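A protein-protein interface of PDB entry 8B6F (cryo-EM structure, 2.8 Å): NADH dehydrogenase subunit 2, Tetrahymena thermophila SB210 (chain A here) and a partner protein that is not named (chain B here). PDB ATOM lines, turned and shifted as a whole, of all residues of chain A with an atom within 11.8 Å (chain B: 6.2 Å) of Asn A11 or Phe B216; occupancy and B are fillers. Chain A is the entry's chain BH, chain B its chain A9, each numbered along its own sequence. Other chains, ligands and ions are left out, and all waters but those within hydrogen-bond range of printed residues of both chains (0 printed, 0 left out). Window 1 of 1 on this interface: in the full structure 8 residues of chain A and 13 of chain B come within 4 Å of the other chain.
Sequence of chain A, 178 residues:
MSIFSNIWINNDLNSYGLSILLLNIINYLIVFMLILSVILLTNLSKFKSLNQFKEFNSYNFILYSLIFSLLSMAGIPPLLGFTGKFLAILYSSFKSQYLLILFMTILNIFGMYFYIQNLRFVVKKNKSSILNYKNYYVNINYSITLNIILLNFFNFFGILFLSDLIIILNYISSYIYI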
ATOM      1  N   MET A   1      -5.919  28.201 -15.687  1.00  0.00           N
ATOM      2  CA  MET A   1      -5.003  27.844 -14.567  1.00  0.00           C
ATOM      3  C   MET A   1      -5.409  26.518 -13.942  1.00  0.00           C
ATOM      4  O   MET A   1      -6.454  26.422 -13.302  1.00  0.00           O
ATOM      5  CB  MET A   1      -5.002  28.938 -13.498  1.00  0.00           C
ATOM      6  CG  MET A   1      -4.595  30.314 -14.008  1.00  0.00           C
ATOM      7  SD  MET A   1      -2.952  30.356 -14.752  1.00  0.00           S
ATOM      8  CE  MET A   1      -1.932  29.779 -13.400  1.00  0.00           C
ATOM      9  N   SER A   2      -4.576  25.497 -14.127  1.00  0.00           N
ATOM     10  CA  SER A   2      -4.813  24.178 -13.566  1.00  0.00           C
ATOM     11  C   SER A   2      -3.551  23.690 -12.872  1.00  0.00           C
ATOM     12  O   SER A   2      -2.435  23.997 -13.297  1.00  0.00           O
ATOM     13  CB  SER A   2      -5.229  23.173 -14.647  1.00  0.00           C
ATOM     14  OG  SER A   2      -6.390  23.611 -15.332  1.00  0.00           O
ATOM     15  N   ILE A   3      -3.738  22.925 -11.801  1.00  0.00           N
ATOM     16  CA  ILE A   3      -2.640  22.406 -10.996  1.00  0.00           C
ATOM     17  C   ILE A   3      -2.670  20.887 -11.080  1.00  0.00           C
ATOM     18  O   ILE A   3      -3.697  20.265 -10.785  1.00  0.00           O
ATOM     19  CB  ILE A   3      -2.741  22.861  -9.528  1.00  0.00           C
ATOM     20  CG1 ILE A   3      -3.099  24.345  -9.450  1.00  0.00           C
ATOM     21  CG2 ILE A   3      -1.422  22.596  -8.817  1.00  0.00           C
ATOM     22  CD1 ILE A   3      -3.281  24.858  -8.034  1.00  0.00           C
ATOM     23  N   PHE A   4      -1.547  20.295 -11.476  1.00  0.00           N
ATOM     24  CA  PHE A   4      -1.395  18.843 -11.545  1.00  0.00           C
ATOM     25  C   PHE A   4      -0.055  18.494 -10.908  1.00  0.00           C
ATOM     26  O   PHE A   4       0.988  18.569 -11.562  1.00  0.00           O
ATOM     27  CB  PHE A   4      -1.475  18.342 -12.985  1.00  0.00           C
ATOM     28  CG  PHE A   4      -2.787  18.632 -13.656  1.00  0.00           C
ATOM     29  CD1 PHE A   4      -3.858  17.768 -13.513  1.00  0.00           C
ATOM     30  CD2 PHE A   4      -2.946  19.765 -14.430  1.00  0.00           C
ATOM     31  CE1 PHE A   4      -5.065  18.032 -14.131  1.00  0.00           C
ATOM     32  CE2 PHE A   4      -4.150  20.033 -15.052  1.00  0.00           C
ATOM     33  CZ  PHE A   4      -5.211  19.167 -14.901  1.00  0.00           C
ATOM     34  N   SER A   5      -0.086  18.110  -9.633  1.00  0.00           N
ATOM     35  CA  SER A   5       1.130  17.806  -8.882  1.00  0.00           C
ATOM     36  C   SER A   5       2.074  19.006  -8.876  1.00  0.00           C
ATOM     37  O   SER A   5       3.263  18.897  -9.181  1.00  0.00           O
ATOM     38  CB  SER A   5       1.824  16.564  -9.446  1.00  0.00           C
ATOM     39  OG  SER A   5       2.987  16.246  -8.699  1.00  0.00           O
ATOM     40  N   ILE A   7       2.277  21.446 -10.842  1.00  0.00           N
ATOM     41  CA  ILE A   7       2.622  21.948 -12.168  1.00  0.00           C
ATOM     42  C   ILE A   7       1.452  22.785 -12.660  1.00  0.00           C
ATOM     43  O   ILE A   7       0.350  22.262 -12.867  1.00  0.00           O
ATOM     44  CB  ILE A   7       2.944  20.807 -13.150  1.00  0.00           C
ATOM     45  CG1 ILE A   7       4.405  20.369 -13.017  1.00  0.00           C
ATOM     46  CG2 ILE A   7       2.679  21.222 -14.595  1.00  0.00           C
ATOM     47  CD1 ILE A   7       4.752  19.757 -11.686  1.00  0.00           C
ATOM     48  N   TRP A   8       1.685  24.081 -12.838  1.00  0.00           N
ATOM     49  CA  TRP A   8       0.643  24.976 -13.314  1.00  0.00           C
ATOM     50  C   TRP A   8       0.523  24.898 -14.829  1.00  0.00           C
ATOM     51  O   TRP A   8       1.525  24.839 -15.545  1.00  0.00           O
ATOM     52  CB  TRP A   8       0.943  26.414 -12.905  1.00  0.00           C
ATOM     53  CG  TRP A   8       0.917  26.617 -11.443  1.00  0.00           C
ATOM     54  CD1 TRP A   8       1.956  26.446 -10.587  1.00  0.00           C
ATOM     55  CD2 TRP A   8      -0.198  27.033 -10.649  1.00  0.00           C
ATOM     56  NE1 TRP A   8       1.564  26.728  -9.309  1.00  0.00           N
ATOM     57  CE2 TRP A   8       0.242  27.091  -9.316  1.00  0.00           C
ATOM     58  CE3 TRP A   8      -1.527  27.360 -10.936  1.00  0.00           C
ATOM     59  CZ2 TRP A   8      -0.596  27.464  -8.269  1.00  0.00           C
ATOM     60  CZ3 TRP A   8      -2.359  27.730  -9.896  1.00  0.00           C
ATOM     61  CH2 TRP A   8      -1.890  27.780  -8.577  1.00  0.00           C
ATOM     62  N   ILE A   9      -0.715  24.892 -15.312  1.00  0.00           N
ATOM     63  CA  ILE A   9      -1.006  24.878 -16.738  1.00  0.00           C
ATOM     64  C   ILE A   9      -1.944  26.038 -17.029  1.00  0.00           C
ATOM     65  O   ILE A   9      -2.999  26.161 -16.399  1.00  0.00           O
ATOM     66  CB  ILE A   9      -1.630  23.544 -17.188  1.00  0.00           C
ATOM     67  CG1 ILE A   9      -0.705  22.388 -16.801  1.00  0.00           C
ATOM     68  CG2 ILE A   9      -1.892  23.562 -18.688  1.00  0.00           C
ATOM     69  CD1 ILE A   9      -1.249  21.025 -17.135  1.00  0.00           C
ATOM     70  N   ASN A  10      -1.562  26.881 -17.983  1.00  0.00           N
ATOM     71  CA  ASN A  10      -2.319  28.079 -18.330  1.00  0.00           C
ATOM     72  C   ASN A  10      -2.657  28.027 -19.813  1.00  0.00           C
ATOM     73  O   ASN A  10      -1.776  28.188 -20.664  1.00  0.00           O
ATOM     74  CB  ASN A  10      -1.533  29.343 -17.984  1.00  0.00           C
ATOM     75  CG  ASN A  10      -0.056  29.214 -18.288  1.00  0.00           C
ATOM     76  OD1 ASN A  10       0.344  28.453 -19.168  1.00  0.00           O
ATOM     77  ND2 ASN A  10       0.765  29.953 -17.552  1.00  0.00           N
ATOM     78  N   ASN A  11      -3.933  27.801 -20.116  1.00  0.00           N
ATOM     79  CA  ASN A  11      -4.437  27.808 -21.480  1.00  0.00           C
ATOM     80  C   ASN A  11      -5.077  29.138 -21.851  1.00  0.00           C
ATOM     81  O   ASN A  11      -5.711  29.235 -22.906  1.00  0.00           O
ATOM     82  CB  ASN A  11      -5.448  26.679 -21.674  1.00  0.00           C
ATOM     83  CG  ASN A  11      -4.859  25.313 -21.390  1.00  0.00           C
ATOM     84  OD1 ASN A  11      -3.650  25.113 -21.486  1.00  0.00           O
ATOM     85  ND2 ASN A  11      -5.716  24.363 -21.038  1.00  0.00           N
ATOM     86  N   ASP A  12      -4.936  30.157 -21.007  1.00  0.00           N
ATOM     87  CA  ASP A  12      -5.507  31.473 -21.249  1.00  0.00           C
ATOM     88  C   ASP A  12      -4.389  32.489 -21.418  1.00  0.00           C
ATOM     89  O   ASP A  12      -3.411  32.483 -20.665  1.00  0.00           O
ATOM     90  CB  ASP A  12      -6.425  31.899 -20.100  1.00  0.00           C
ATOM     91  CG  ASP A  12      -7.563  30.926 -19.871  1.00  0.00           C
ATOM     92  OD1 ASP A  12      -7.997  30.278 -20.847  1.00  0.00           O
ATOM     93  OD2 ASP A  12      -8.025  30.806 -18.718  1.00  0.00           O
ATOM     94  N   LEU A  13      -4.539  33.358 -22.412  1.00  0.00           N
ATOM     95  CA  LEU A  13      -3.590  34.432 -22.679  1.00  0.00           C
ATOM     96  C   LEU A  13      -4.150  35.707 -22.062  1.00  0.00           C
ATOM     97  O   LEU A  13      -5.132  36.266 -22.560  1.00  0.00           O
ATOM     98  CB  LEU A  13      -3.361  34.593 -24.180  1.00  0.00           C
ATOM     99  CG  LEU A  13      -2.314  35.624 -24.609  1.00  0.00           C
ATOM    100  CD1 LEU A  13      -0.928  35.210 -24.146  1.00  0.00           C
ATOM    101  CD2 LEU A  13      -2.344  35.811 -26.115  1.00  0.00           C
ATOM    102  N   ASN A  14      -3.525  36.165 -20.975  1.00  0.00           N
ATOM    103  CA  ASN A  14      -4.065  37.304 -20.243  1.00  0.00           C
ATOM    104  C   ASN A  14      -4.039  38.571 -21.088  1.00  0.00           C
ATOM    105  O   ASN A  14      -4.970  39.382 -21.032  1.00  0.00           O
ATOM    106  CB  ASN A  14      -3.279  37.508 -18.948  1.00  0.00           C
ATOM    107  CG  ASN A  14      -3.993  38.416 -17.974  1.00  0.00           C
ATOM    108  OD1 ASN A  14      -5.105  38.872 -18.235  1.00  0.00           O
ATOM    109  ND2 ASN A  14      -3.362  38.676 -16.837  1.00  0.00           N
ATOM    110  N   SER A  15      -2.980  38.761 -21.872  1.00  0.00           N
ATOM    111  CA  SER A  15      -2.828  39.956 -22.699  1.00  0.00           C
ATOM    112  C   SER A  15      -3.563  39.779 -24.030  1.00  0.00           C
ATOM    113  O   SER A  15      -2.983  39.840 -25.114  1.00  0.00           O
ATOM    114  CB  SER A  15      -1.352  40.245 -22.925  1.00  0.00           C
ATOM    115  OG  SER A  15      -0.745  39.170 -23.620  1.00  0.00           O
ATOM    116  N   TYR A  16      -4.866  39.560 -23.928  1.00  0.00           N
ATOM    117  CA  TYR A  16      -5.730  39.404 -25.091  1.00  0.00           C
ATOM    118  C   TYR A  16      -6.877  40.397 -25.110  1.00  0.00           C
ATOM    119  O   TYR A  16      -7.241  40.890 -26.178  1.00  0.00           O
ATOM    120  CB  TYR A  16      -6.292  37.975 -25.144  1.00  0.00           C
ATOM    121  CG  TYR A  16      -6.978  37.647 -26.450  1.00  0.00           C
ATOM    122  CD1 TYR A  16      -8.335  37.883 -26.622  1.00  0.00           C
ATOM    123  CD2 TYR A  16      -6.268  37.104 -27.511  1.00  0.00           C
ATOM    124  CE1 TYR A  16      -8.967  37.588 -27.815  1.00  0.00           C
ATOM    125  CE2 TYR A  16      -6.888  36.807 -28.708  1.00  0.00           C
ATOM    126  CZ  TYR A  16      -8.237  37.050 -28.853  1.00  0.00           C
ATOM    127  OH  TYR A  16      -8.859  36.755 -30.042  1.00  0.00           O
ATOM    128  N   GLY A  17      -7.459  40.705 -23.951  1.00  0.00           N
ATOM    129  CA  GLY A  17      -8.494  41.722 -23.904  1.00  0.00           C
ATOM    130  C   GLY A  17      -7.982  43.090 -24.306  1.00  0.00           C
ATOM    131  O   GLY A  17      -8.669  43.843 -24.999  1.00  0.00           O
ATOM    132  N   TYR A  91     -14.848  37.896 -26.677  1.00  0.00           N
ATOM    133  CA  TYR A  91     -14.087  38.026 -25.441  1.00  0.00           C
ATOM    134  C   TYR A  91     -15.009  38.111 -24.230  1.00  0.00           C
ATOM    135  O   TYR A  91     -14.698  37.561 -23.168  1.00  0.00           O
ATOM    136  CB  TYR A  91     -13.174  39.248 -25.511  1.00  0.00           C
ATOM    137  CG  TYR A  91     -12.239  39.357 -24.332  1.00  0.00           C
ATOM    138  CD1 TYR A  91     -11.162  38.494 -24.193  1.00  0.00           C
ATOM    139  CD2 TYR A  91     -12.431  40.326 -23.360  1.00  0.00           C
ATOM    140  CE1 TYR A  91     -10.307  38.589 -23.118  1.00  0.00           C
ATOM    141  CE2 TYR A  91     -11.584  40.431 -22.282  1.00  0.00           C
ATOM    142  CZ  TYR A  91     -10.522  39.561 -22.165  1.00  0.00           C
ATOM    143  OH  TYR A  91      -9.674  39.664 -21.090  1.00  0.00           O
ATOM    144  N   PHE A  94     -15.960  34.664 -23.525  1.00  0.00           N
ATOM    145  CA  PHE A  94     -14.819  33.978 -22.930  1.00  0.00           C
ATOM    146  C   PHE A  94     -14.682  34.326 -21.455  1.00  0.00           C
ATOM    147  O   PHE A  94     -14.371  33.459 -20.630  1.00  0.00           O
ATOM    148  CB  PHE A  94     -13.546  34.342 -23.695  1.00  0.00           C
ATOM    149  CG  PHE A  94     -12.333  33.582 -23.252  1.00  0.00           C
ATOM    150  CD1 PHE A  94     -12.110  32.294 -23.700  1.00  0.00           C
ATOM    151  CD2 PHE A  94     -11.404  34.162 -22.406  1.00  0.00           C
ATOM    152  CE1 PHE A  94     -10.994  31.593 -23.304  1.00  0.00           C
ATOM    153  CE2 PHE A  94     -10.284  33.465 -22.007  1.00  0.00           C
ATOM    154  CZ  PHE A  94     -10.079  32.178 -22.456  1.00  0.00           C
ATOM    155  N   LYS A  95     -14.915  35.589 -21.103  1.00  0.00           N
ATOM    156  CA  LYS A  95     -14.884  36.030 -19.715  1.00  0.00           C
ATOM    157  C   LYS A  95     -16.174  35.716 -18.972  1.00  0.00           C
ATOM    158  O   LYS A  95     -16.258  35.991 -17.771  1.00  0.00           O
ATOM    159  CB  LYS A  95     -14.604  37.533 -19.647  1.00  0.00           C
ATOM    160  CG  LYS A  95     -13.318  37.954 -20.345  1.00  0.00           C
ATOM    161  CD  LYS A  95     -12.075  37.505 -19.590  1.00  0.00           C
ATOM    162  CE  LYS A  95     -11.839  38.361 -18.359  1.00  0.00           C
ATOM    163  NZ  LYS A  95     -10.577  38.004 -17.660  1.00  0.00           N
ATOM    164  N   ASN A 170      -1.577  41.517 -30.396  1.00  0.00           N
ATOM    165  CA  ASN A 170      -1.249  40.656 -29.265  1.00  0.00           C
ATOM    166  C   ASN A 170       0.237  40.715 -28.946  1.00  0.00           C
ATOM    167  O   ASN A 170       0.634  40.678 -27.778  1.00  0.00           O
ATOM    168  CB  ASN A 170      -1.676  39.220 -29.555  1.00  0.00           C
ATOM    169  CG  ASN A 170      -3.156  39.004 -29.341  1.00  0.00           C
ATOM    170  OD1 ASN A 170      -3.578  38.551 -28.280  1.00  0.00           O
ATOM    171  ND2 ASN A 170      -3.957  39.332 -30.348  1.00  0.00           N
ATOM    172  N   LYS B 211      -3.060  10.854 -12.993  1.00  0.00           N
ATOM    173  CA  LYS B 211      -4.156  10.341 -13.807  1.00  0.00           C
ATOM    174  C   LYS B 211      -5.042  11.474 -14.304  1.00  0.00           C
ATOM    175  O   LYS B 211      -5.480  11.471 -15.460  1.00  0.00           O
ATOM    176  CB  LYS B 211      -4.980   9.334 -13.008  1.00  0.00           C
ATOM    177  CG  LYS B 211      -4.314   7.982 -12.839  1.00  0.00           C
ATOM    178  CD  LYS B 211      -5.282   6.975 -12.249  1.00  0.00           C
ATOM    179  CE  LYS B 211      -4.680   5.584 -12.206  1.00  0.00           C
ATOM    180  NZ  LYS B 211      -5.672   4.579 -11.732  1.00  0.00           N
ATOM    181  N   ASP B 212      -5.322  12.450 -13.439  1.00  0.00           N
ATOM    182  CA  ASP B 212      -6.142  13.587 -13.844  1.00  0.00           C
ATOM    183  C   ASP B 212      -5.466  14.382 -14.950  1.00  0.00           C
ATOM    184  O   ASP B 212      -6.127  14.843 -15.886  1.00  0.00           O
ATOM    185  CB  ASP B 212      -6.430  14.486 -12.643  1.00  0.00           C
ATOM    186  CG  ASP B 212      -7.380  13.848 -11.655  1.00  0.00           C
ATOM    187  OD1 ASP B 212      -7.873  12.736 -11.935  1.00  0.00           O
ATOM    188  OD2 ASP B 212      -7.638  14.459 -10.597  1.00  0.00           O
ATOM    189  N   TYR B 213      -4.147  14.549 -14.862  1.00  0.00           N
ATOM    190  CA  TYR B 213      -3.428  15.243 -15.922  1.00  0.00           C
ATOM    191  C   TYR B 213      -3.487  14.469 -17.233  1.00  0.00           C
ATOM    192  O   TYR B 213      -3.649  15.064 -18.305  1.00  0.00           O
ATOM    193  CB  TYR B 213      -1.974  15.469 -15.512  1.00  0.00           C
ATOM    194  CG  TYR B 213      -1.162  16.050 -16.634  1.00  0.00           C
ATOM    195  CD1 TYR B 213      -1.358  17.363 -17.034  1.00  0.00           C
ATOM    196  CD2 TYR B 213      -0.222  15.288 -17.311  1.00  0.00           C
ATOM    197  CE1 TYR B 213      -0.636  17.907 -18.061  1.00  0.00           C
ATOM    198  CE2 TYR B 213       0.509  15.825 -18.349  1.00  0.00           C
ATOM    199  CZ  TYR B 213       0.288  17.138 -18.719  1.00  0.00           C
ATOM    200  OH  TYR B 213       0.999  17.701 -19.743  1.00  0.00           O
ATOM    201  N   ILE B 214      -3.359  13.143 -17.174  1.00  0.00           N
ATOM    202  CA  ILE B 214      -3.458  12.340 -18.390  1.00  0.00           C
ATOM    203  C   ILE B 214      -4.831  12.516 -19.024  1.00  0.00           C
ATOM    204  O   ILE B 214      -4.954  12.643 -20.248  1.00  0.00           O
ATOM    205  CB  ILE B 214      -3.153  10.862 -18.081  1.00  0.00           C
ATOM    206  CG1 ILE B 214      -1.686  10.682 -17.678  1.00  0.00           C
ATOM    207  CG2 ILE B 214      -3.488   9.974 -19.277  1.00  0.00           C
ATOM    208  CD1 ILE B 214      -0.675  11.041 -18.752  1.00  0.00           C
ATOM    209  N   GLN B 215      -5.886  12.516 -18.208  1.00  0.00           N
ATOM    210  CA  GLN B 215      -7.220  12.774 -18.735  1.00  0.00           C
ATOM    211  C   GLN B 215      -7.312  14.180 -19.312  1.00  0.00           C
ATOM    212  O   GLN B 215      -7.896  14.386 -20.382  1.00  0.00           O
ATOM    213  CB  GLN B 215      -8.272  12.577 -17.645  1.00  0.00           C
ATOM    214  CG  GLN B 215      -9.689  12.856 -18.121  1.00  0.00           C
ATOM    215  CD  GLN B 215     -10.728  12.569 -17.063  1.00  0.00           C
ATOM    216  OE1 GLN B 215     -10.402  12.258 -15.920  1.00  0.00           O
ATOM    217  NE2 GLN B 215     -11.997  12.670 -17.442  1.00  0.00           N
ATOM    218  N   PHE B 216      -6.741  15.162 -18.611  1.00  0.00           N
ATOM    219  CA  PHE B 216      -6.797  16.545 -19.069  1.00  0.00           C
ATOM    220  C   PHE B 216      -6.121  16.715 -20.421  1.00  0.00           C
ATOM    221  O   PHE B 216      -6.550  17.548 -21.226  1.00  0.00           O
ATOM    222  CB  PHE B 216      -6.146  17.453 -18.024  1.00  0.00           C
ATOM    223  CG  PHE B 216      -5.665  18.764 -18.568  1.00  0.00           C
ATOM    224  CD1 PHE B 216      -6.538  19.827 -18.721  1.00  0.00           C
ATOM    225  CD2 PHE B 216      -4.333  18.942 -18.902  1.00  0.00           C
ATOM    226  CE1 PHE B 216      -6.095  21.038 -19.213  1.00  0.00           C
ATOM    227  CE2 PHE B 216      -3.884  20.150 -19.392  1.00  0.00           C
ATOM    228  CZ  PHE B 216      -4.766  21.199 -19.549  1.00  0.00           C
ATOM    229  N   LEU B 217      -5.068  15.941 -20.691  1.00  0.00           N
ATOM    230  CA  LEU B 217      -4.400  16.028 -21.985  1.00  0.00           C
ATOM    231  C   LEU B 217      -5.389  15.856 -23.128  1.00  0.00           C
ATOM    232  O   LEU B 217      -5.281  16.529 -24.158  1.00  0.00           O
ATOM    233  CB  LEU B 217      -3.291  14.978 -22.076  1.00  0.00           C
ATOM    234  CG  LEU B 217      -2.002  15.284 -21.309  1.00  0.00           C
ATOM    235  CD1 LEU B 217      -1.063  14.097 -21.357  1.00  0.00           C
ATOM    236  CD2 LEU B 217      -1.312  16.518 -21.865  1.00  0.00           C
ATOM    237  N   GLY B 218      -6.381  14.984 -22.953  1.00  0.00           N
ATOM    238  CA  GLY B 218      -7.359  14.753 -24.001  1.00  0.00           C
ATOM    239  C   GLY B 218      -8.158  15.983 -24.373  1.00  0.00           C
ATOM    240  O   GLY B 218      -8.783  16.005 -25.438  1.00  0.00           O
ATOM    241  N   ASN B 219      -8.160  17.010 -23.521  1.00  0.00           N
ATOM    242  CA  ASN B 219      -8.877  18.236 -23.851  1.00  0.00           C
ATOM    243  C   ASN B 219      -8.291  18.900 -25.090  1.00  0.00           C
ATOM    244  O   ASN B 219      -9.033  19.414 -25.935  1.00  0.00           O
ATOM    245  CB  ASN B 219      -8.847  19.199 -22.666  1.00  0.00           C
ATOM    246  CG  ASN B 219      -9.734  18.747 -21.527  1.00  0.00           C
ATOM    247  OD1 ASN B 219     -10.198  17.608 -21.499  1.00  0.00           O
ATOM    248  ND2 ASN B 219      -9.977  19.641 -20.576  1.00  0.00           N
ATOM    249  N   TYR B 220      -6.966  18.907 -25.213  1.00  0.00           N
ATOM    250  CA  TYR B 220      -6.330  19.504 -26.379  1.00  0.00           C
ATOM    251  C   TYR B 220      -6.808  18.821 -27.653  1.00  0.00           C
ATOM    252  O   TYR B 220      -6.865  17.591 -27.731  1.00  0.00           O
ATOM    253  CB  TYR B 220      -4.810  19.398 -26.256  1.00  0.00           C
ATOM    254  CG  TYR B 220      -4.244  20.251 -25.153  1.00  0.00           C
ATOM    255  CD1 TYR B 220      -4.139  21.624 -25.298  1.00  0.00           C
ATOM    256  CD2 TYR B 220      -3.817  19.682 -23.962  1.00  0.00           C
ATOM    257  CE1 TYR B 220      -3.627  22.408 -24.291  1.00  0.00           C
ATOM    258  CE2 TYR B 220      -3.304  20.457 -22.949  1.00  0.00           C
ATOM    259  CZ  TYR B 220      -3.217  21.821 -23.117  1.00  0.00           C
ATOM    260  OH  TYR B 220      -2.703  22.597 -22.110  1.00  0.00           O
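Of the 10 printed residues of chain B, 4 touch a printed residue of chain A. Hydrophobic or aromatic side chains of chain B within 4 Å of the printed part of chain A: Tyr B213, Phe B216 and Tyr B220. Of the 20 printed residues of chain A, 3 touch a printed residue of chain B. Printed residues of chain A that touch a printed residue of chain B: Phe A4, Ile A9 and Asn A11. Hydrophobic or aromatic side chains of chain A within 4 Å of the printed part of chain B: Phe A4 and Ile A9. Among the printed residues, 8 pairs touch across the chains. Among the printed residues, no Asp or Glu carboxylate lies within 4 Å of a Lys or Arg side-chain nitrogen of the other chain.
N of Ile A9 lies within hydrogen-bond range of O of Ser A2 (2.8 Å).
Phe A4 touches Asp B212 (CE1 to C, 3.8 Å). Tyr B213 touches Phe A4. Phe A4 touches Phe B216 (CZ to CB, 3.7 Å). Ile A9 touches Tyr B213 (CD1 to CE1, 3.3 Å). CD1 of Ile A9 touches CE2 of Phe B216, 3.6 Å away. CG2 of Ile A9 touches OH of Tyr B220, 3.6 Å away. Phe B216 touches Asn A11.
Printed residues of chain B within 4 Å of Phe A4: Asp B212 (3.8 Å), Tyr B213 (3.5 Å) and Phe B216 (3.7 Å). Of the printed residues of chain B, Ile A9 touches Tyr B213 (3.3 Å), Phe B216 (3.6 Å) and Tyr B220 (3.6 Å). Of the printed residues of chain A, Asp B212 touches Phe A4 (3.8 Å). No residue of chain A comes within 4 Å of Ile B214. No residue of chain A comes within 4 Å of Gln B215. Of the printed residues of chain A, Phe B216 touches Phe A4, Ile A9 and Asn A11. Leu B217 touches none of the printed residues of chain A. Asn B219 touches none of the printed residues of chain A. Of chain A, only Ile A9 and Asn A11 come within 4 Å of Tyr B220.
The side-chain amide oxygen (OD1) of Asn A11 lies within hydrogen-bond range of the side-chain hydroxyl (OH) of Tyr B220 (2.8 Å).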
